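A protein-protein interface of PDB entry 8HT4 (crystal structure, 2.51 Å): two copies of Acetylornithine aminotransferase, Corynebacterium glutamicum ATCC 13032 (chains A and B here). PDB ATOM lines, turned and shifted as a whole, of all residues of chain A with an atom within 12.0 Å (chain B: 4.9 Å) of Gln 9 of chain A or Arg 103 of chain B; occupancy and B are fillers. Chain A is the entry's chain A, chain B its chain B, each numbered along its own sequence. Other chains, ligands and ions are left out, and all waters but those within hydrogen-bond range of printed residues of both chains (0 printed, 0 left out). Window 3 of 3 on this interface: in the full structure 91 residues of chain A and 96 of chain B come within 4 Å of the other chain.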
ATOM      1  N   THR A   3      17.137  14.437   0.011  1.00  0.00           N
ATOM      2  CA  THR A   3      17.249  13.149  -0.748  1.00  0.00           C
ATOM      3  C   THR A   3      16.487  13.274  -2.070  1.00  0.00           C
ATOM      4  O   THR A   3      17.128  13.531  -3.081  1.00  0.00           O
ATOM      5  CB  THR A   3      16.724  11.953   0.056  1.00  0.00           C
ATOM      6  OG1 THR A   3      15.361  12.229   0.399  1.00  0.00           O
ATOM      7  CG2 THR A   3      17.574  11.649   1.274  1.00  0.00           C
ATOM      8  N   LEU A   4      15.162  13.158  -2.042  1.00  0.00           N
ATOM      9  CA  LEU A   4      14.277  13.416  -3.216  1.00  0.00           C
ATOM     10  C   LEU A   4      14.504  14.824  -3.806  1.00  0.00           C
ATOM     11  O   LEU A   4      14.438  14.954  -5.024  1.00  0.00           O
ATOM     12  CB  LEU A   4      12.818  13.227  -2.777  1.00  0.00           C
ATOM     13  CG  LEU A   4      12.412  11.782  -2.497  1.00  0.00           C
ATOM     14  CD1 LEU A   4      11.074  11.707  -1.754  1.00  0.00           C
ATOM     15  CD2 LEU A   4      12.371  10.993  -3.799  1.00  0.00           C
ATOM     16  N   GLU A   5      14.747  15.845  -2.981  1.00  0.00           N
ATOM     17  CA  GLU A   5      14.982  17.247  -3.432  1.00  0.00           C
ATOM     18  C   GLU A   5      16.297  17.329  -4.222  1.00  0.00           C
ATOM     19  O   GLU A   5      16.346  18.065  -5.239  1.00  0.00           O
ATOM     20  CB  GLU A   5      14.989  18.190  -2.227  1.00  0.00           C
ATOM     21  CG  GLU A   5      13.634  18.257  -1.554  1.00  0.00           C
ATOM     22  CD  GLU A   5      13.550  18.933  -0.197  1.00  0.00           C
ATOM     23  OE1 GLU A   5      14.598  19.359   0.309  1.00  0.00           O
ATOM     24  OE2 GLU A   5      12.413  19.014   0.354  1.00  0.00           O
ATOM     25  N   THR A   6      17.315  16.580  -3.787  1.00  0.00           N
ATOM     26  CA  THR A   6      18.692  16.628  -4.343  1.00  0.00           C
ATOM     27  C   THR A   6      18.880  15.464  -5.324  1.00  0.00           C
ATOM     28  O   THR A   6      19.890  15.460  -6.028  1.00  0.00           O
ATOM     29  CB  THR A   6      19.729  16.771  -3.216  1.00  0.00           C
ATOM     30  OG1 THR A   6      20.984  16.421  -3.785  1.00  0.00           O
ATOM     31  CG2 THR A   6      19.477  15.918  -1.994  1.00  0.00           C
ATOM     32  N   TRP A   7      17.902  14.565  -5.440  1.00  0.00           N
ATOM     33  CA  TRP A   7      17.909  13.411  -6.387  1.00  0.00           C
ATOM     34  C   TRP A   7      17.902  13.924  -7.832  1.00  0.00           C
ATOM     35  O   TRP A   7      18.780  13.571  -8.611  1.00  0.00           O
ATOM     36  CB  TRP A   7      16.737  12.458  -6.080  1.00  0.00           C
ATOM     37  CG  TRP A   7      16.937  11.020  -6.464  1.00  0.00           C
ATOM     38  CD1 TRP A   7      17.280   9.971  -5.654  1.00  0.00           C
ATOM     39  CD2 TRP A   7      16.759  10.457  -7.770  1.00  0.00           C
ATOM     40  NE1 TRP A   7      17.343   8.800  -6.364  1.00  0.00           N
ATOM     41  CE2 TRP A   7      17.039   9.071  -7.668  1.00  0.00           C
ATOM     42  CE3 TRP A   7      16.410  11.001  -9.006  1.00  0.00           C
ATOM     43  CZ2 TRP A   7      16.986   8.216  -8.762  1.00  0.00           C
ATOM     44  CZ3 TRP A   7      16.359  10.156 -10.088  1.00  0.00           C
ATOM     45  CH2 TRP A   7      16.628   8.785  -9.962  1.00  0.00           C
ATOM     46  N   PRO A   8      16.950  14.786  -8.266  1.00  0.00           N
ATOM     47  CA  PRO A   8      16.922  15.240  -9.662  1.00  0.00           C
ATOM     48  C   PRO A   8      18.030  16.244 -10.062  1.00  0.00           C
ATOM     49  O   PRO A   8      18.209  16.446 -11.264  1.00  0.00           O
ATOM     50  CB  PRO A   8      15.521  15.878  -9.798  1.00  0.00           C
ATOM     51  CG  PRO A   8      15.224  16.382  -8.410  1.00  0.00           C
ATOM     52  CD  PRO A   8      15.864  15.374  -7.472  1.00  0.00           C
ATOM     53  N   GLN A   9      18.747  16.847  -9.096  1.00  0.00           N
ATOM     54  CA  GLN A   9      19.865  17.800  -9.376  1.00  0.00           C
ATOM     55  C   GLN A   9      21.158  17.023  -9.687  1.00  0.00           C
ATOM     56  O   GLN A   9      22.110  17.656 -10.151  1.00  0.00           O
ATOM     57  CB  GLN A   9      20.133  18.747  -8.196  1.00  0.00           C
ATOM     58  CG  GLN A   9      19.021  19.748  -7.873  1.00  0.00           C
ATOM     59  CD  GLN A   9      19.130  20.312  -6.468  1.00  0.00           C
ATOM     60  OE1 GLN A   9      20.022  19.962  -5.680  1.00  0.00           O
ATOM     61  NE2 GLN A   9      18.208  21.198  -6.123  1.00  0.00           N
ATOM     62  N   VAL A  10      21.206  15.708  -9.429  1.00  0.00           N
ATOM     63  CA  VAL A  10      22.464  14.899  -9.472  1.00  0.00           C
ATOM     64  C   VAL A  10      22.291  13.562 -10.238  1.00  0.00           C
ATOM     65  O   VAL A  10      23.300  13.039 -10.792  1.00  0.00           O
ATOM     66  CB  VAL A  10      22.978  14.721  -8.029  1.00  0.00           C
ATOM     67  CG1 VAL A  10      23.169  16.065  -7.337  1.00  0.00           C
ATOM     68  CG2 VAL A  10      22.068  13.838  -7.197  1.00  0.00           C
ATOM     69  N   ILE A  11      21.085  12.999 -10.304  1.00  0.00           N
ATOM     70  CA  ILE A  11      20.862  11.658 -10.916  1.00  0.00           C
ATOM     71  C   ILE A  11      20.388  11.882 -12.348  1.00  0.00           C
ATOM     72  O   ILE A  11      19.480  12.700 -12.511  1.00  0.00           O
ATOM     73  CB  ILE A  11      19.887  10.817 -10.065  1.00  0.00           C
ATOM     74  CG1 ILE A  11      20.475  10.593  -8.671  1.00  0.00           C
ATOM     75  CG2 ILE A  11      19.528   9.506 -10.748  1.00  0.00           C
ATOM     76  CD1 ILE A  11      21.864   9.994  -8.684  1.00  0.00           C
ATOM     77  N   ILE A  12      21.018  11.229 -13.332  1.00  0.00           N
ATOM     78  CA  ILE A  12      20.578  11.293 -14.761  1.00  0.00           C
ATOM     79  C   ILE A  12      19.116  10.830 -14.813  1.00  0.00           C
ATOM     80  O   ILE A  12      18.766   9.799 -14.150  1.00  0.00           O
ATOM     81  CB  ILE A  12      21.509  10.496 -15.707  1.00  0.00           C
ATOM     82  CG1 ILE A  12      22.843  11.232 -15.928  1.00  0.00           C
ATOM     83  CG2 ILE A  12      20.808  10.210 -17.030  1.00  0.00           C
ATOM     84  CD1 ILE A  12      23.858  10.508 -16.796  1.00  0.00           C
ATOM     85  N   ASN A  13      18.286  11.598 -15.524  1.00  0.00           N
ATOM     86  CA  ASN A  13      16.807  11.443 -15.524  1.00  0.00           C
ATOM     87  C   ASN A  13      16.439  10.268 -16.439  1.00  0.00           C
ATOM     88  O   ASN A  13      15.922  10.488 -17.556  1.00  0.00           O
ATOM     89  CB  ASN A  13      16.059  12.725 -15.893  1.00  0.00           C
ATOM     90  CG  ASN A  13      14.576  12.572 -15.619  1.00  0.00           C
ATOM     91  OD1 ASN A  13      14.203  11.977 -14.608  1.00  0.00           O
ATOM     92  ND2 ASN A  13      13.738  13.047 -16.529  1.00  0.00           N
ATOM     93  N   THR A  14      16.730   9.064 -15.950  1.00  0.00           N
ATOM     94  CA  THR A  14      16.622   7.777 -16.671  1.00  0.00           C
ATOM     95  C   THR A  14      15.432   7.003 -16.072  1.00  0.00           C
ATOM     96  O   THR A  14      14.879   6.103 -16.771  1.00  0.00           O
ATOM     97  CB  THR A  14      17.998   7.102 -16.612  1.00  0.00           C
ATOM     98  OG1 THR A  14      18.179   6.224 -17.723  1.00  0.00           O
ATOM     99  CG2 THR A  14      18.206   6.343 -15.323  1.00  0.00           C
ATOM    100  N   TYR A  15      15.023   7.372 -14.851  1.00  0.00           N
ATOM    101  CA  TYR A  15      13.976   6.685 -14.047  1.00  0.00           C
ATOM    102  C   TYR A  15      12.867   7.661 -13.602  1.00  0.00           C
ATOM    103  O   TYR A  15      11.975   7.246 -12.838  1.00  0.00           O
ATOM    104  CB  TYR A  15      14.619   6.036 -12.821  1.00  0.00           C
ATOM    105  CG  TYR A  15      15.820   5.172 -13.095  1.00  0.00           C
ATOM    106  CD1 TYR A  15      15.694   3.956 -13.756  1.00  0.00           C
ATOM    107  CD2 TYR A  15      17.082   5.531 -12.634  1.00  0.00           C
ATOM    108  CE1 TYR A  15      16.789   3.128 -13.969  1.00  0.00           C
ATOM    109  CE2 TYR A  15      18.191   4.722 -12.846  1.00  0.00           C
ATOM    110  CZ  TYR A  15      18.041   3.512 -13.510  1.00  0.00           C
ATOM    111  OH  TYR A  15      19.119   2.704 -13.731  1.00  0.00           O
ATOM    112  N   GLY A  16      12.892   8.912 -14.077  1.00  0.00           N
ATOM    113  CA  GLY A  16      12.173  10.034 -13.443  1.00  0.00           C
ATOM    114  C   GLY A  16      12.695  10.240 -12.030  1.00  0.00           C
ATOM    115  O   GLY A  16      13.792   9.726 -11.724  1.00  0.00           O
ATOM    116  N   THR A  17      11.935  10.966 -11.205  1.00  0.00           N
ATOM    117  CA  THR A  17      12.179  11.171  -9.750  1.00  0.00           C
ATOM    118  C   THR A  17      11.308  10.171  -8.999  1.00  0.00           C
ATOM    119  O   THR A  17      10.089  10.143  -9.173  1.00  0.00           O
ATOM    120  CB  THR A  17      11.927  12.625  -9.320  1.00  0.00           C
ATOM    121  OG1 THR A  17      12.775  13.489 -10.081  1.00  0.00           O
ATOM    122  CG2 THR A  17      12.185  12.845  -7.844  1.00  0.00           C
ATOM    123  N   PRO A  18      11.912   9.280  -8.186  1.00  0.00           N
ATOM    124  CA  PRO A  18      11.135   8.378  -7.335  1.00  0.00           C
ATOM    125  C   PRO A  18      10.144   9.110  -6.430  1.00  0.00           C
ATOM    126  O   PRO A  18      10.456  10.175  -5.900  1.00  0.00           O
ATOM    127  CB  PRO A  18      12.222   7.688  -6.497  1.00  0.00           C
ATOM    128  CG  PRO A  18      13.464   7.750  -7.366  1.00  0.00           C
ATOM    129  CD  PRO A  18      13.364   9.089  -8.059  1.00  0.00           C
ATOM    130  N   ILE B  88      30.031  14.955  -8.478  1.00  0.00           N
ATOM    131  CA  ILE B  88      29.737  16.202  -9.247  1.00  0.00           C
ATOM    132  C   ILE B  88      30.558  17.350  -8.655  1.00  0.00           C
ATOM    133  O   ILE B  88      31.111  18.144  -9.448  1.00  0.00           O
ATOM    134  CB  ILE B  88      28.226  16.515  -9.248  1.00  0.00           C
ATOM    135  CG1 ILE B  88      27.429  15.438  -9.990  1.00  0.00           C
ATOM    136  CG2 ILE B  88      27.964  17.901  -9.822  1.00  0.00           C
ATOM    137  CD1 ILE B  88      25.948  15.516  -9.778  1.00  0.00           C
ATOM    138  N   ALA B  99      28.348  22.239 -12.311  1.00  0.00           N
ATOM    139  CA  ALA B  99      27.763  21.274 -11.351  1.00  0.00           C
ATOM    140  C   ALA B  99      26.269  21.128 -11.620  1.00  0.00           C
ATOM    141  O   ALA B  99      25.746  20.008 -11.477  1.00  0.00           O
ATOM    142  CB  ALA B  99      28.005  21.708  -9.929  1.00  0.00           C
ATOM    143  N   ALA B 100      25.598  22.228 -11.952  1.00  0.00           N
ATOM    144  CA  ALA B 100      24.127  22.273 -12.096  1.00  0.00           C
ATOM    145  C   ALA B 100      23.705  21.612 -13.417  1.00  0.00           C
ATOM    146  O   ALA B 100      22.530  21.309 -13.559  1.00  0.00           O
ATOM    147  CB  ALA B 100      23.645  23.699 -11.998  1.00  0.00           C
ATOM    148  N   GLN B 101      24.646  21.421 -14.339  1.00  0.00           N
ATOM    149  CA  GLN B 101      24.422  20.904 -15.715  1.00  0.00           C
ATOM    150  C   GLN B 101      24.883  19.445 -15.814  1.00  0.00           C
ATOM    151  O   GLN B 101      24.715  18.864 -16.909  1.00  0.00           O
ATOM    152  CB  GLN B 101      25.192  21.767 -16.720  1.00  0.00           C
ATOM    153  CG  GLN B 101      24.686  23.208 -16.805  1.00  0.00           C
ATOM    154  CD  GLN B 101      25.355  23.999 -17.909  1.00  0.00           C
ATOM    155  OE1 GLN B 101      24.904  25.083 -18.291  1.00  0.00           O
ATOM    156  NE2 GLN B 101      26.446  23.456 -18.434  1.00  0.00           N
ATOM    157  N   THR B 102      25.472  18.938 -14.717  1.00  0.00           N
ATOM    158  CA  THR B 102      26.023  17.562 -14.656  1.00  0.00           C
ATOM    159  C   THR B 102      25.151  16.608 -13.842  1.00  0.00           C
ATOM    160  O   THR B 102      24.608  17.031 -12.822  1.00  0.00           O
ATOM    161  CB  THR B 102      27.534  17.492 -14.359  1.00  0.00           C
ATOM    162  OG1 THR B 102      27.910  16.122 -14.237  1.00  0.00           O
ATOM    163  CG2 THR B 102      27.984  18.182 -13.107  1.00  0.00           C
ATOM    164  N   ARG B 103      25.062  15.367 -14.305  1.00  0.00           N
ATOM    165  CA  ARG B 103      24.248  14.303 -13.679  1.00  0.00           C
ATOM    166  C   ARG B 103      25.076  13.007 -13.730  1.00  0.00           C
ATOM    167  O   ARG B 103      25.971  12.896 -14.584  1.00  0.00           O
ATOM    168  CB  ARG B 103      22.905  14.106 -14.414  1.00  0.00           C
ATOM    169  CG  ARG B 103      21.970  15.305 -14.465  1.00  0.00           C
ATOM    170  CD  ARG B 103      21.512  15.742 -13.083  1.00  0.00           C
ATOM    171  NE  ARG B 103      20.546  16.849 -13.105  1.00  0.00           N
ATOM    172  CZ  ARG B 103      20.840  18.152 -13.154  1.00  0.00           C
ATOM    173  NH1 ARG B 103      22.098  18.553 -13.196  1.00  0.00           N
ATOM    174  NH2 ARG B 103      19.871  19.048 -13.173  1.00  0.00           N
ATOM    175  N   VAL B 104      24.743  12.048 -12.871  1.00  0.00           N
ATOM    176  CA  VAL B 104      25.426  10.731 -12.807  1.00  0.00           C
ATOM    177  C   VAL B 104      24.378   9.611 -12.919  1.00  0.00           C
ATOM    178  O   VAL B 104      23.378   9.656 -12.199  1.00  0.00           O
ATOM    179  CB  VAL B 104      26.272  10.630 -11.522  1.00  0.00           C
ATOM    180  CG1 VAL B 104      26.945   9.274 -11.387  1.00  0.00           C
ATOM    181  CG2 VAL B 104      27.298  11.751 -11.465  1.00  0.00           C
ATOM    182  N   PHE B 105      24.620   8.652 -13.815  1.00  0.00           N
ATOM    183  CA  PHE B 105      23.946   7.330 -13.863  1.00  0.00           C
ATOM    184  C   PHE B 105      24.863   6.301 -13.194  1.00  0.00           C
ATOM    185  O   PHE B 105      26.025   6.197 -13.628  1.00  0.00           O
ATOM    186  CB  PHE B 105      23.615   6.946 -15.309  1.00  0.00           C
ATOM    187  CG  PHE B 105      23.311   5.486 -15.509  1.00  0.00           C
ATOM    188  CD1 PHE B 105      22.029   4.996 -15.329  1.00  0.00           C
ATOM    189  CD2 PHE B 105      24.304   4.599 -15.889  1.00  0.00           C
ATOM    190  CE1 PHE B 105      21.740   3.657 -15.549  1.00  0.00           C
ATOM    191  CE2 PHE B 105      24.022   3.259 -16.098  1.00  0.00           C
ATOM    192  CZ  PHE B 105      22.737   2.786 -15.931  1.00  0.00           C
ATOM    193  N   CYS B 264      28.643   6.684 -14.729  1.00  0.00           N
ATOM    194  CA  CYS B 264      28.767   7.470 -15.961  1.00  0.00           C
ATOM    195  C   CYS B 264      28.274   8.879 -15.621  1.00  0.00           C
ATOM    196  O   CYS B 264      27.060   9.074 -15.389  1.00  0.00           O
ATOM    197  CB  CYS B 264      28.011   6.802 -17.099  1.00  0.00           C
ATOM    198  SG  CYS B 264      28.171   7.768 -18.609  1.00  0.00           S
ATOM    199  N   LEU B 265      29.208   9.803 -15.502  1.00  0.00           N
ATOM    200  CA  LEU B 265      28.885  11.217 -15.272  1.00  0.00           C
ATOM    201  C   LEU B 265      28.747  11.874 -16.648  1.00  0.00           C
ATOM    202  O   LEU B 265      29.534  11.540 -17.539  1.00  0.00           O
ATOM    203  CB  LEU B 265      30.029  11.759 -14.417  1.00  0.00           C
ATOM    204  CG  LEU B 265      29.908  13.188 -13.918  1.00  0.00           C
ATOM    205  CD1 LEU B 265      30.385  13.290 -12.472  1.00  0.00           C
ATOM    206  CD2 LEU B 265      30.726  14.114 -14.818  1.00  0.00           C
ATOM    207  N   ALA B 266      27.715  12.690 -16.841  1.00  0.00           N
ATOM    208  CA  ALA B 266      27.507  13.481 -18.065  1.00  0.00           C
ATOM    209  C   ALA B 266      27.180  14.914 -17.670  1.00  0.00           C
ATOM    210  O   ALA B 266      26.519  15.102 -16.652  1.00  0.00           O
ATOM    211  CB  ALA B 266      26.417  12.867 -18.897  1.00  0.00           C
ATOM    212  N   ALA B 271      24.132  15.010 -20.735  1.00  0.00           N
ATOM    213  CA  ALA B 271      23.271  14.749 -19.561  1.00  0.00           C
ATOM    214  C   ALA B 271      21.820  14.676 -20.016  1.00  0.00           C
ATOM    215  O   ALA B 271      21.098  13.871 -19.444  1.00  0.00           O
ATOM    216  CB  ALA B 271      23.450  15.807 -18.502  1.00  0.00           C
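No position is printed for both chains.
Of the 13 pairs that touch across the chains among the printed residues, none has its exchanged pair printed and touching as well.
Of the 16 printed residues of chain A, 6 touch a printed residue of chain B.
Hydrophobic or aromatic side chains of chain A that line the printed part of chain B: Val 10, Ile 11, Ile 12 and Tyr 15.
Hydrophobic or aromatic side chains of chain B that line the printed part of chain A: Ile 88, Val 104 and Phe 105.
Along chain B the printed residues that touch a printed residue of chain A span positions 88 to 264.
The backbone NH of Ile 12 of chain A lies within hydrogen-bond range of the backbone carbonyl oxygen of Val 104 of chain B, 3.1 Å away.
NH1 of Arg 103 of chain B sits at hydrogen-bond distance from O of Gln 9 of chain A (3.2 Å).
N of Val 104 of chain B sits at hydrogen-bond distance from O of Val 10 of chain A (2.7 Å).
The backbone carbonyl oxygen (O) of Pro 8 of chain A sits at hydrogen-bond distance from the guanidinium group (NE) of Arg 103 of chain B, 3.0 Å away.
OG1 of Thr 102 of chain B lies within hydrogen-bond range of O of Ala 266 of chain B (3.0 Å).
The backbone carbonyl oxygen (O) of Phe 105 of chain B lies within hydrogen-bond range of the backbone NH (N) of Cys 264 of chain B (2.9 Å).
The backbone carbonyl oxygen of Ala 266 of chain B is in hydrogen-bond range of the backbone NH of Arg 103 of chain B (2.8 Å).
The backbone carbonyl oxygen (O) of Ala 100 of chain B lies within hydrogen-bond range of the guanidinium group (NH1) of Arg 103 of chain B.
Thr 102 of chain B touches Gln 9 of chain A (O to O, 3.7 Å).
CB of Val 10 of chain A touches CD1 of Ile 88 of chain B (3.5 Å).
Val 10 of chain A touches Arg 103 of chain B (O to CA, 3.3 Å).
Ile 11 of chain A touches Arg 103 of chain B.
Val 104 of chain B touches Ile 11 of chain A.
Ile 12 of chain A touches Arg 103 of chain B (CG1 to CB, 3.2 Å).
CD1 of Ile 12 of chain A touches N of Phe 105 of chain B, at 3.6 Å.
Ile 12 of chain A touches Cys 264 of chain B.
Tyr 15 of chain A touches Phe 105 of chain B.
Printed residues of chain B within 4 Å of Pro 8 of chain A: Arg 103.
Gln 9 of chain A touches just these residues of chain B: Thr 102 (3.7 Å) and Arg 103 (3.2 Å).
Printed residues of chain B within 4 Å of Val 10 of chain A: Ile 88 (3.5 Å), Arg 103 (3.3 Å) and Val 104 (2.7 Å).
Of the printed residues of chain B, Ile 11 of chain A touches Arg 103 and Val 104.
Thr 14 of chain A touches none of the printed residues of chain B.
Of the printed residues of chain B, Tyr 15 of chain A touches Phe 105.
No residue of chain A comes within 4 Å of Ala 99 of chain B.
No residue of chain A comes within 4 Å of Ala 100 of chain B.
Of chain A, only Gln 9 (3.7 Å) comes within 4 Å of Thr 102 of chain B.
Arg 103 of chain B touches five residues of chain A.
Of the printed residues of chain A, Val 104 of chain B touches Val 10 (2.7 Å), Ile 11 (3.5 Å) and Ile 12 (3.1 Å).
Of the printed residues of chain A, Phe 105 of chain B touches Ile 12 and Tyr 15.
Leu 265 of chain B touches none of the printed residues of chain A.
No residue of chain A comes within 4 Å of Ala 266 of chain B.
The nearest residue of chain A that does not touch Arg 103 of chain B is Asn 13 of chain A (5.3 Å).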
